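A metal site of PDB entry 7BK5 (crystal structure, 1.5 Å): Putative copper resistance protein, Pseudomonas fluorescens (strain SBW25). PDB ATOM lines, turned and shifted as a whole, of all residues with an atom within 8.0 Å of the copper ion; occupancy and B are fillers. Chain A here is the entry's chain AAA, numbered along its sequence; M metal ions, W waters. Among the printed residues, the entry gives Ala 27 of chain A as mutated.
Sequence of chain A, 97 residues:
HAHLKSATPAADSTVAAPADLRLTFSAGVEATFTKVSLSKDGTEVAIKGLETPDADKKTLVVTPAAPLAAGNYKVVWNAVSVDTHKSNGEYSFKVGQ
OG of Ser 81 is in hydrogen-bond range of O of His 85, 3.0 Å away.
Within 4 Å of the copper ion: His 1, Asp 83 and His 85.
The copper ion is bound by a ring nitrogen (ND1) of His 85 (1.9 Å), the backbone nitrogen (N) of His 1 (2.2 Å), a ring nitrogen (ND1) of His 1 (2.3 Å), water W1 (2.5 Å) and the side-chain carboxylate (OD2) of Asp 83 (2.5 Å).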
ATOM      1  N   HIS A   1      15.691  -0.594  11.541  1.00  0.00           N
ATOM      2  CA  HIS A   1      16.690  -1.648  11.249  1.00  0.00           C
ATOM      3  C   HIS A   1      18.070  -1.146  11.652  1.00  0.00           C
ATOM      4  O   HIS A   1      18.301   0.056  11.566  1.00  0.00           O
ATOM      5  CB  HIS A   1      16.746  -2.031   9.765  1.00  0.00           C
ATOM      6  CG  HIS A   1      15.690  -3.012   9.414  1.00  0.00           C
ATOM      7  ND1 HIS A   1      14.355  -2.749   9.633  1.00  0.00           N
ATOM      8  CD2 HIS A   1      15.772  -4.262   8.897  1.00  0.00           C
ATOM      9  CE1 HIS A   1      13.646  -3.790   9.260  1.00  0.00           C
ATOM     10  NE2 HIS A   1      14.490  -4.735   8.799  1.00  0.00           N
ATOM     11  N   ALA A   2      18.925  -2.071  12.063  1.00  0.00           N
ATOM     12  CA  ALA A   2      20.332  -1.790  12.400  1.00  0.00           C
ATOM     13  C   ALA A   2      21.192  -2.526  11.383  1.00  0.00           C
ATOM     14  O   ALA A   2      21.098  -3.752  11.299  1.00  0.00           O
ATOM     15  CB  ALA A   2      20.619  -2.212  13.822  1.00  0.00           C
ATOM     16  N   HIS A   3      21.911  -1.777  10.543  1.00  0.00           N
ATOM     17  CA  HIS A   3      22.876  -2.326   9.564  1.00  0.00           C
ATOM     18  C   HIS A   3      24.274  -2.209  10.139  1.00  0.00           C
ATOM     19  O   HIS A   3      24.531  -1.158  10.726  1.00  0.00           O
ATOM     20  CB  HIS A   3      22.724  -1.553   8.238  1.00  0.00           C
ATOM     21  CG  HIS A   3      21.295  -1.372   7.866  1.00  0.00           C
ATOM     22  ND1 HIS A   3      20.542  -2.412   7.366  1.00  0.00           N
ATOM     23  CD2 HIS A   3      20.455  -0.317   7.976  1.00  0.00           C
ATOM     24  CE1 HIS A   3      19.321  -1.986   7.144  1.00  0.00           C
ATOM     25  NE2 HIS A   3      19.231  -0.711   7.524  1.00  0.00           N
ATOM     26  N   ALA A  27      21.913   1.963  13.818  1.00  0.00           N
ATOM     27  CA  ALA A  27      20.917   2.342  14.835  1.00  0.00           C
ATOM     28  C   ALA A  27      21.245   1.549  16.083  1.00  0.00           C
ATOM     29  O   ALA A  27      21.992   0.580  15.962  1.00  0.00           O
ATOM     30  CB  ALA A  27      19.517   2.037  14.383  1.00  0.00           C
ATOM     31  N   SER A  81      17.208  -4.373  16.806  1.00  0.00           N
ATOM     32  CA  SER A  81      17.327  -2.905  16.962  1.00  0.00           C
ATOM     33  C   SER A  81      16.346  -2.418  18.033  1.00  0.00           C
ATOM     34  O   SER A  81      15.476  -3.187  18.481  1.00  0.00           O
ATOM     35  CB  SER A  81      17.105  -2.220  15.654  1.00  0.00           C
ATOM     36  OG  SER A  81      15.903  -2.670  15.058  1.00  0.00           O
ATOM     37  N   VAL A  82      16.492  -1.161  18.458  1.00  0.00           N
ATOM     38  CA  VAL A  82      15.613  -0.563  19.488  1.00  0.00           C
ATOM     39  C   VAL A  82      14.172  -0.503  18.980  1.00  0.00           C
ATOM     40  O   VAL A  82      13.308  -0.341  19.833  1.00  0.00           O
ATOM     41  CB  VAL A  82      16.122   0.818  19.934  1.00  0.00           C
ATOM     42  CG1 VAL A  82      17.405   0.692  20.732  1.00  0.00           C
ATOM     43  CG2 VAL A  82      16.311   1.784  18.781  1.00  0.00           C
ATOM     44  N   ASP A  83      13.941  -0.589  17.660  1.00  0.00           N
ATOM     45  CA  ASP A  83      12.576  -0.595  17.058  1.00  0.00           C
ATOM     46  C   ASP A  83      12.028  -2.035  16.999  1.00  0.00           C
ATOM     47  O   ASP A  83      10.882  -2.243  16.474  1.00  0.00           O
ATOM     48  CB  ASP A  83      12.544   0.081  15.683  1.00  0.00           C
ATOM     49  CG  ASP A  83      13.296  -0.618  14.553  1.00  0.00           C
ATOM     50  OD1 ASP A  83      13.779  -1.741  14.764  1.00  0.00           O
ATOM     51  OD2 ASP A  83      13.374  -0.027  13.436  1.00  0.00           O
ATOM     52  N   THR A  84      12.781  -2.988  17.544  1.00  0.00           N
ATOM     53  CA  THR A  84      12.428  -4.445  17.617  1.00  0.00           C
ATOM     54  C   THR A  84      12.697  -5.146  16.280  1.00  0.00           C
ATOM     55  O   THR A  84      12.490  -6.335  16.270  1.00  0.00           O
ATOM     56  CB  THR A  84      10.984  -4.720  18.061  1.00  0.00           C
ATOM     57  OG1 THR A  84      10.059  -4.456  16.990  1.00  0.00           O
ATOM     58  CG2 THR A  84      10.573  -3.928  19.284  1.00  0.00           C
ATOM     59  N   HIS A  85      13.209  -4.484  15.247  1.00  0.00           N
ATOM     60  CA  HIS A  85      13.466  -5.096  13.904  1.00  0.00           C
ATOM     61  C   HIS A  85      14.736  -5.952  13.902  1.00  0.00           C
ATOM     62  O   HIS A  85      15.711  -5.590  14.585  1.00  0.00           O
ATOM     63  CB  HIS A  85      13.516  -4.077  12.752  1.00  0.00           C
ATOM     64  CG  HIS A  85      12.227  -3.359  12.604  1.00  0.00           C
ATOM     65  ND1 HIS A  85      12.101  -2.228  11.831  1.00  0.00           N
ATOM     66  CD2 HIS A  85      11.002  -3.579  13.162  1.00  0.00           C
ATOM     67  CE1 HIS A  85      10.858  -1.775  11.921  1.00  0.00           C
ATOM     68  NE2 HIS A  85      10.174  -2.589  12.716  1.00  0.00           N
ATOM     69  N   LYS A  86      14.708  -7.030  13.124  1.00  0.00           N
ATOM     70  CA  LYS A  86      15.796  -8.036  13.096  1.00  0.00           C
ATOM     71  C   LYS A  86      16.611  -7.843  11.826  1.00  0.00           C
ATOM     72  O   LYS A  86      16.014  -7.596  10.756  1.00  0.00           O
ATOM     73  CB  LYS A  86      15.269  -9.468  13.239  1.00  0.00           C
ATOM     74  CG  LYS A  86      14.152  -9.625  14.278  1.00  0.00           C
ATOM     75  CD  LYS A  86      14.297 -10.777  15.244  1.00  0.00           C
ATOM     76  CE  LYS A  86      14.621 -12.105  14.633  1.00  0.00           C
ATOM     77  NZ  LYS A  86      14.588 -13.179  15.665  1.00  0.00           N
ATOM     78  N   SER A  87      17.923  -7.973  11.940  1.00  0.00           N
ATOM     79  CA  SER A  87      18.910  -7.992  10.849  1.00  0.00           C
ATOM     80  C   SER A  87      19.960  -9.056  11.171  1.00  0.00           C
ATOM     81  O   SER A  87      20.040  -9.482  12.367  1.00  0.00           O
ATOM     82  CB  SER A  87      19.531  -6.641  10.622  1.00  0.00           C
ATOM     83  OG  SER A  87      20.180  -6.194  11.803  1.00  0.00           O
HETATM   84 CU    CU M   1      13.669  -1.394  11.305  1.00  0.00          CU
HETATM   85  O   HOH W   1      13.058   0.468   9.767  1.00  0.00           O
